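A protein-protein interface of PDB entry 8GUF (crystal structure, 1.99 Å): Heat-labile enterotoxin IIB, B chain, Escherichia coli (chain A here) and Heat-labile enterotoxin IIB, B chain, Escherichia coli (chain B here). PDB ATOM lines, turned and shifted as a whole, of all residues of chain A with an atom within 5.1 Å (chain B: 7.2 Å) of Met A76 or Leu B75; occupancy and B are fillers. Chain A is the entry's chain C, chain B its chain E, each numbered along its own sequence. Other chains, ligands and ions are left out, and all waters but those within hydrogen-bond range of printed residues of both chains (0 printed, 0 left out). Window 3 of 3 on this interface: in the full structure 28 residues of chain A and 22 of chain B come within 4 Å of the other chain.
The backbone NH of Ala A98 sits at hydrogen-bond distance from the backbone carbonyl oxygen of Thr B26 (2.9 Å).
The backbone carbonyl oxygen of Arg A77 sits at hydrogen-bond distance from the backbone NH of Glu A97 (3.0 Å).
The side-chain hydroxyl of Ser A74 sits close to the side-chain sulfur of Met A76, at 3.3 Å.
SD of Met A76 touches CD2 of Leu B75, 3.0 Å away.
O of Leu A96 touches O of Thr B26 (3.6 Å).
Thr B26 touches Glu A97.
CB of Ala A98 touches O of Val B74 (3.3 Å).
Of the printed residues of chain B, Met A76 touches Leu B75.
Leu B75 touches just one residue of chain A: Met A76 (3.0 Å).
No residue of chain B comes within 4 Å of Gly A75.
Printed residues of chain B within 4 Å of Glu A97: Thr B26.
Of the printed residues of chain B, Ala A98 touches Thr B26 (2.9 Å) and Val B74 (3.3 Å).
Printed residues of chain A within 4 Å of Thr B26: Leu A96 (3.6 Å), Glu A97 (3.6 Å) and Ala A98 (2.9 Å).
Printed residues of chain A within 4 Å of Val B74: Ala A98.
Printed residues of chain B within 4 Å of Leu A96: Thr B26.
Gly B77 touches none of the printed residues of chain A.
Ala A70 touches none of the printed residues of chain B.
The nearest residue of chain B that does not touch Met A76 is Val B74 (4.04 Å).
Printed residues of chain A that touch a printed residue of chain B: Met A76, Leu A96, Glu A97 and Ala A98.
Hydrophobic or aromatic side chains of chain A within 4 Å of the printed part of chain B: Met A76 and Ala A98.
Along chain A the printed residues that touch a printed residue of chain B span positions 76 to 98.
Hydrophobic or aromatic side chains of chain B within 4 Å of the printed part of chain A: Leu B75.
Among the printed residues, 5 pairs touch across the chains.
Among the printed residues, no Asp or Glu carboxylate lies within 4 Å of a Lys or Arg side-chain nitrogen of the other chain.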
ATOM      1  N   VAL A  21     -12.388 -12.406  29.850  1.00  0.00           N
ATOM      2  CA  VAL A  21     -11.332 -11.494  29.466  1.00  0.00           C
ATOM      3  C   VAL A  21     -11.881 -10.428  28.528  1.00  0.00           C
ATOM      4  O   VAL A  21     -12.608 -10.734  27.583  1.00  0.00           O
ATOM      5  CB  VAL A  21     -10.149 -12.225  28.805  1.00  0.00           C
ATOM      6  CG1 VAL A  21      -9.108 -11.218  28.344  1.00  0.00           C
ATOM      7  CG2 VAL A  21      -9.526 -13.256  29.728  1.00  0.00           C
ATOM      8  N   ALA A  70     -13.625  -9.613  16.717  1.00  0.00           N
ATOM      9  CA  ALA A  70     -15.002  -9.302  17.086  1.00  0.00           C
ATOM     10  C   ALA A  70     -15.047  -8.887  18.550  1.00  0.00           C
ATOM     11  O   ALA A  70     -15.843  -8.030  18.930  1.00  0.00           O
ATOM     12  CB  ALA A  70     -15.913 -10.468  16.820  1.00  0.00           C
ATOM     13  N   ALA A  71     -14.164  -9.474  19.356  1.00  0.00           N
ATOM     14  CA  ALA A  71     -14.075  -9.110  20.758  1.00  0.00           C
ATOM     15  C   ALA A  71     -13.582  -7.677  20.903  1.00  0.00           C
ATOM     16  O   ALA A  71     -14.169  -6.885  21.637  1.00  0.00           O
ATOM     17  CB  ALA A  71     -13.197 -10.083  21.512  1.00  0.00           C
ATOM     18  N   SER A  74     -16.150  -5.018  19.488  1.00  0.00           N
ATOM     19  CA  SER A  74     -17.475  -4.933  20.071  1.00  0.00           C
ATOM     20  C   SER A  74     -17.436  -4.964  21.599  1.00  0.00           C
ATOM     21  O   SER A  74     -18.453  -4.699  22.233  1.00  0.00           O
ATOM     22  CB  SER A  74     -18.325  -6.049  19.547  1.00  0.00           C
ATOM     23  OG  SER A  74     -17.959  -7.275  20.166  1.00  0.00           O
ATOM     24  N   GLY A  75     -16.293  -5.347  22.193  1.00  0.00           N
ATOM     25  CA  GLY A  75     -16.174  -5.459  23.642  1.00  0.00           C
ATOM     26  C   GLY A  75     -16.909  -6.662  24.245  1.00  0.00           C
ATOM     27  O   GLY A  75     -17.134  -6.711  25.455  1.00  0.00           O
ATOM     28  N   MET A  76     -17.300  -7.635  23.420  1.00  0.00           N
ATOM     29  CA  MET A  76     -17.807  -8.896  23.929  1.00  0.00           C
ATOM     30  C   MET A  76     -16.644  -9.595  24.609  1.00  0.00           C
ATOM     31  O   MET A  76     -15.500  -9.426  24.182  1.00  0.00           O
ATOM     32  CB  MET A  76     -18.298  -9.797  22.802  1.00  0.00           C
ATOM     33  CG  MET A  76     -19.490  -9.261  22.083  1.00  0.00           C
ATOM     34  SD  MET A  76     -19.598 -10.075  20.476  1.00  0.00           S
ATOM     35  CE  MET A  76     -20.378 -11.603  20.979  1.00  0.00           C
ATOM     36  N   ARG A  77     -16.929 -10.357  25.665  1.00  0.00           N
ATOM     37  CA  ARG A  77     -15.844 -10.964  26.421  1.00  0.00           C
ATOM     38  C   ARG A  77     -15.584 -12.379  25.902  1.00  0.00           C
ATOM     39  O   ARG A  77     -16.407 -12.936  25.168  1.00  0.00           O
ATOM     40  CB  ARG A  77     -16.105 -10.807  27.929  1.00  0.00           C
ATOM     41  CG  ARG A  77     -15.467  -9.525  28.472  1.00  0.00           C
ATOM     42  CD  ARG A  77     -16.385  -8.597  29.246  1.00  0.00           C
ATOM     43  NE  ARG A  77     -16.449  -7.278  28.630  1.00  0.00           N
ATOM     44  CZ  ARG A  77     -16.381  -6.099  29.243  1.00  0.00           C
ATOM     45  NH1 ARG A  77     -16.372  -5.994  30.558  1.00  0.00           N
ATOM     46  NH2 ARG A  77     -16.332  -5.003  28.513  1.00  0.00           N
ATOM     47  N   VAL A  78     -14.391 -12.892  26.243  1.00  0.00           N
ATOM     48  CA  VAL A  78     -13.934 -14.207  25.824  1.00  0.00           C
ATOM     49  C   VAL A  78     -13.490 -15.021  27.042  1.00  0.00           C
ATOM     50  O   VAL A  78     -13.105 -14.455  28.055  1.00  0.00           O
ATOM     51  CB  VAL A  78     -12.806 -14.090  24.779  1.00  0.00           C
ATOM     52  CG1 VAL A  78     -13.255 -13.257  23.592  1.00  0.00           C
ATOM     53  CG2 VAL A  78     -11.514 -13.534  25.367  1.00  0.00           C
ATOM     54  N   LEU A  96     -16.218 -17.197  22.526  1.00  0.00           N
ATOM     55  CA  LEU A  96     -16.830 -15.882  22.368  1.00  0.00           C
ATOM     56  C   LEU A  96     -18.198 -15.860  23.050  1.00  0.00           C
ATOM     57  O   LEU A  96     -19.072 -16.682  22.748  1.00  0.00           O
ATOM     58  CB  LEU A  96     -16.965 -15.536  20.879  1.00  0.00           C
ATOM     59  CG  LEU A  96     -17.501 -14.134  20.564  1.00  0.00           C
ATOM     60  CD1 LEU A  96     -16.563 -13.032  21.066  1.00  0.00           C
ATOM     61  CD2 LEU A  96     -17.749 -13.966  19.078  1.00  0.00           C
ATOM     62  N   GLU A  97     -18.384 -14.910  23.968  1.00  0.00           N
ATOM     63  CA  GLU A  97     -19.649 -14.779  24.684  1.00  0.00           C
ATOM     64  C   GLU A  97     -20.522 -13.665  24.093  1.00  0.00           C
ATOM     65  O   GLU A  97     -20.074 -12.532  23.926  1.00  0.00           O
ATOM     66  CB  GLU A  97     -19.407 -14.438  26.156  1.00  0.00           C
ATOM     67  CG  GLU A  97     -18.525 -15.424  26.906  1.00  0.00           C
ATOM     68  CD  GLU A  97     -18.307 -15.012  28.360  1.00  0.00           C
ATOM     69  OE1 GLU A  97     -18.456 -15.860  29.263  1.00  0.00           O
ATOM     70  OE2 GLU A  97     -18.018 -13.818  28.596  1.00  0.00           O
ATOM     71  N   ALA A  98     -21.811 -13.962  23.875  1.00  0.00           N
ATOM     72  CA  ALA A  98     -22.743 -12.983  23.316  1.00  0.00           C
ATOM     73  C   ALA A  98     -22.945 -11.845  24.311  1.00  0.00           C
ATOM     74  O   ALA A  98     -23.056 -12.102  25.512  1.00  0.00           O
ATOM     75  CB  ALA A  98     -24.057 -13.642  22.979  1.00  0.00           C
ATOM     76  N   GLU A  99     -23.030 -10.605  23.802  1.00  0.00           N
ATOM     77  CA  GLU A  99     -23.502  -9.464  24.582  1.00  0.00           C
ATOM     78  C   GLU A  99     -24.787  -9.850  25.319  1.00  0.00           C
ATOM     79  O   GLU A  99     -25.672 -10.484  24.747  1.00  0.00           O
ATOM     80  CB  GLU A  99     -23.822  -8.246  23.711  1.00  0.00           C
ATOM     81  CG  GLU A  99     -23.215  -6.941  24.207  1.00  0.00           C
ATOM     82  CD  GLU A  99     -21.912  -6.582  23.499  1.00  0.00           C
ATOM     83  OE1 GLU A  99     -21.919  -6.518  22.242  1.00  0.00           O
ATOM     84  OE2 GLU A  99     -20.892  -6.354  24.187  1.00  0.00           O
ATOM     85  N   LEU B  25     -28.038 -18.850  20.111  1.00  0.00           N
ATOM     86  CA  LEU B  25     -26.655 -19.228  20.346  1.00  0.00           C
ATOM     87  C   LEU B  25     -25.959 -18.116  21.121  1.00  0.00           C
ATOM     88  O   LEU B  25     -26.004 -16.947  20.732  1.00  0.00           O
ATOM     89  CB  LEU B  25     -25.962 -19.485  19.000  1.00  0.00           C
ATOM     90  CG  LEU B  25     -26.528 -20.610  18.135  1.00  0.00           C
ATOM     91  CD1 LEU B  25     -25.624 -20.835  16.931  1.00  0.00           C
ATOM     92  CD2 LEU B  25     -26.688 -21.920  18.911  1.00  0.00           C
ATOM     93  N   THR B  26     -25.285 -18.474  22.217  1.00  0.00           N
ATOM     94  CA  THR B  26     -24.651 -17.450  23.042  1.00  0.00           C
ATOM     95  C   THR B  26     -23.144 -17.659  23.216  1.00  0.00           C
ATOM     96  O   THR B  26     -22.467 -16.796  23.793  1.00  0.00           O
ATOM     97  CB  THR B  26     -25.337 -17.372  24.412  1.00  0.00           C
ATOM     98  OG1 THR B  26     -25.135 -18.627  25.034  1.00  0.00           O
ATOM     99  CG2 THR B  26     -26.830 -17.145  24.330  1.00  0.00           C
ATOM    100  N   LYS B  68     -20.076 -18.688   9.535  1.00  0.00           N
ATOM    101  CA  LYS B  68     -20.467 -17.288   9.439  1.00  0.00           C
ATOM    102  C   LYS B  68     -21.860 -17.062  10.039  1.00  0.00           C
ATOM    103  O   LYS B  68     -22.071 -16.069  10.719  1.00  0.00           O
ATOM    104  CB  LYS B  68     -20.444 -16.830   7.976  1.00  0.00           C
ATOM    105  CG  LYS B  68     -19.058 -16.808   7.338  1.00  0.00           C
ATOM    106  CD  LYS B  68     -19.078 -16.396   5.883  1.00  0.00           C
ATOM    107  CE  LYS B  68     -17.696 -16.315   5.262  1.00  0.00           C
ATOM    108  NZ  LYS B  68     -17.832 -16.094   3.796  1.00  0.00           N
ATOM    109  N   ILE B  69     -22.797 -17.981   9.763  1.00  0.00           N
ATOM    110  CA  ILE B  69     -24.113 -18.005  10.383  1.00  0.00           C
ATOM    111  C   ILE B  69     -23.983 -18.155  11.907  1.00  0.00           C
ATOM    112  O   ILE B  69     -24.592 -17.384  12.652  1.00  0.00           O
ATOM    113  CB  ILE B  69     -24.983 -19.114   9.750  1.00  0.00           C
ATOM    114  CG1 ILE B  69     -25.311 -18.805   8.290  1.00  0.00           C
ATOM    115  CG2 ILE B  69     -26.232 -19.334  10.581  1.00  0.00           C
ATOM    116  CD1 ILE B  69     -25.909 -19.969   7.518  1.00  0.00           C
ATOM    117  N   ALA B  70     -23.191 -19.122  12.393  1.00  0.00           N
ATOM    118  CA  ALA B  70     -23.013 -19.292  13.832  1.00  0.00           C
ATOM    119  C   ALA B  70     -22.524 -18.011  14.484  1.00  0.00           C
ATOM    120  O   ALA B  70     -23.057 -17.610  15.525  1.00  0.00           O
ATOM    121  CB  ALA B  70     -22.037 -20.393  14.138  1.00  0.00           C
ATOM    122  N   MET B  71     -21.484 -17.388  13.898  1.00  0.00           N
ATOM    123  CA  MET B  71     -20.919 -16.211  14.534  1.00  0.00           C
ATOM    124  C   MET B  71     -21.881 -15.020  14.453  1.00  0.00           C
ATOM    125  O   MET B  71     -21.976 -14.245  15.408  1.00  0.00           O
ATOM    126  CB  MET B  71     -19.565 -15.789  13.970  1.00  0.00           C
ATOM    127  CG  MET B  71     -18.983 -14.647  14.814  1.00  0.00           C
ATOM    128  SD  MET B  71     -17.195 -14.504  14.771  1.00  0.00           S
ATOM    129  CE  MET B  71     -16.827 -15.583  13.392  1.00  0.00           C
ATOM    130  N   ALA B  72     -22.546 -14.834  13.311  1.00  0.00           N
ATOM    131  CA  ALA B  72     -23.522 -13.759  13.197  1.00  0.00           C
ATOM    132  C   ALA B  72     -24.658 -13.932  14.209  1.00  0.00           C
ATOM    133  O   ALA B  72     -25.159 -12.928  14.718  1.00  0.00           O
ATOM    134  CB  ALA B  72     -24.066 -13.669  11.795  1.00  0.00           C
ATOM    135  N   ALA B  73     -25.107 -15.175  14.469  1.00  0.00           N
ATOM    136  CA  ALA B  73     -26.159 -15.405  15.456  1.00  0.00           C
ATOM    137  C   ALA B  73     -25.668 -14.984  16.834  1.00  0.00           C
ATOM    138  O   ALA B  73     -26.427 -14.334  17.569  1.00  0.00           O
ATOM    139  CB  ALA B  73     -26.642 -16.834  15.480  1.00  0.00           C
ATOM    140  N   VAL B  74     -24.393 -15.307  17.139  1.00  0.00           N
ATOM    141  CA  VAL B  74     -23.804 -15.025  18.444  1.00  0.00           C
ATOM    142  C   VAL B  74     -23.696 -13.513  18.654  1.00  0.00           C
ATOM    143  O   VAL B  74     -24.125 -13.018  19.698  1.00  0.00           O
ATOM    144  CB  VAL B  74     -22.453 -15.742  18.680  1.00  0.00           C
ATOM    145  CG1 VAL B  74     -21.793 -15.254  19.966  1.00  0.00           C
ATOM    146  CG2 VAL B  74     -22.593 -17.252  18.751  1.00  0.00           C
ATOM    147  N   LEU B  75     -23.191 -12.786  17.637  1.00  0.00           N
ATOM    148  CA  LEU B  75     -23.040 -11.338  17.699  1.00  0.00           C
ATOM    149  C   LEU B  75     -24.403 -10.641  17.757  1.00  0.00           C
ATOM    150  O   LEU B  75     -24.536  -9.674  18.497  1.00  0.00           O
ATOM    151  CB  LEU B  75     -22.236 -10.825  16.495  1.00  0.00           C
ATOM    152  CG  LEU B  75     -20.787 -11.310  16.397  1.00  0.00           C
ATOM    153  CD1 LEU B  75     -20.129 -10.828  15.111  1.00  0.00           C
ATOM    154  CD2 LEU B  75     -19.975 -10.858  17.597  1.00  0.00           C
ATOM    155  N   SER B  76     -25.392 -11.127  16.994  1.00  0.00           N
ATOM    156  CA  SER B  76     -26.599 -10.355  16.710  1.00  0.00           C
ATOM    157  C   SER B  76     -27.773 -10.717  17.625  1.00  0.00           C
ATOM    158  O   SER B  76     -28.661  -9.895  17.822  1.00  0.00           O
ATOM    159  CB  SER B  76     -27.000 -10.464  15.267  1.00  0.00           C
ATOM    160  OG  SER B  76     -27.427 -11.782  14.963  1.00  0.00           O
ATOM    161  N   GLY B  77     -27.779 -11.917  18.201  1.00  0.00           N
ATOM    162  CA  GLY B  77     -28.931 -12.382  18.953  1.00  0.00           C
ATOM    163  C   GLY B  77     -29.947 -13.078  18.054  1.00  0.00           C
ATOM    164  O   GLY B  77     -30.927 -13.622  18.543  1.00  0.00           O
ATOM    165  N   MET B  78     -29.692 -13.131  16.744  1.00  0.00           N
ATOM    166  CA  MET B  78     -30.640 -13.776  15.846  1.00  0.00           C
ATOM    167  C   MET B  78     -30.707 -15.275  16.126  1.00  0.00           C
ATOM    168  O   MET B  78     -29.719 -15.915  16.457  1.00  0.00           O
ATOM    169  CB  MET B  78     -30.267 -13.530  14.380  1.00  0.00           C
ATOM    170  CG  MET B  78     -30.527 -12.100  13.948  1.00  0.00           C
ATOM    171  SD  MET B  78     -29.674 -11.730  12.380  1.00  0.00           S
ATOM    172  CE  MET B  78     -30.759 -12.591  11.246  1.00  0.00           C
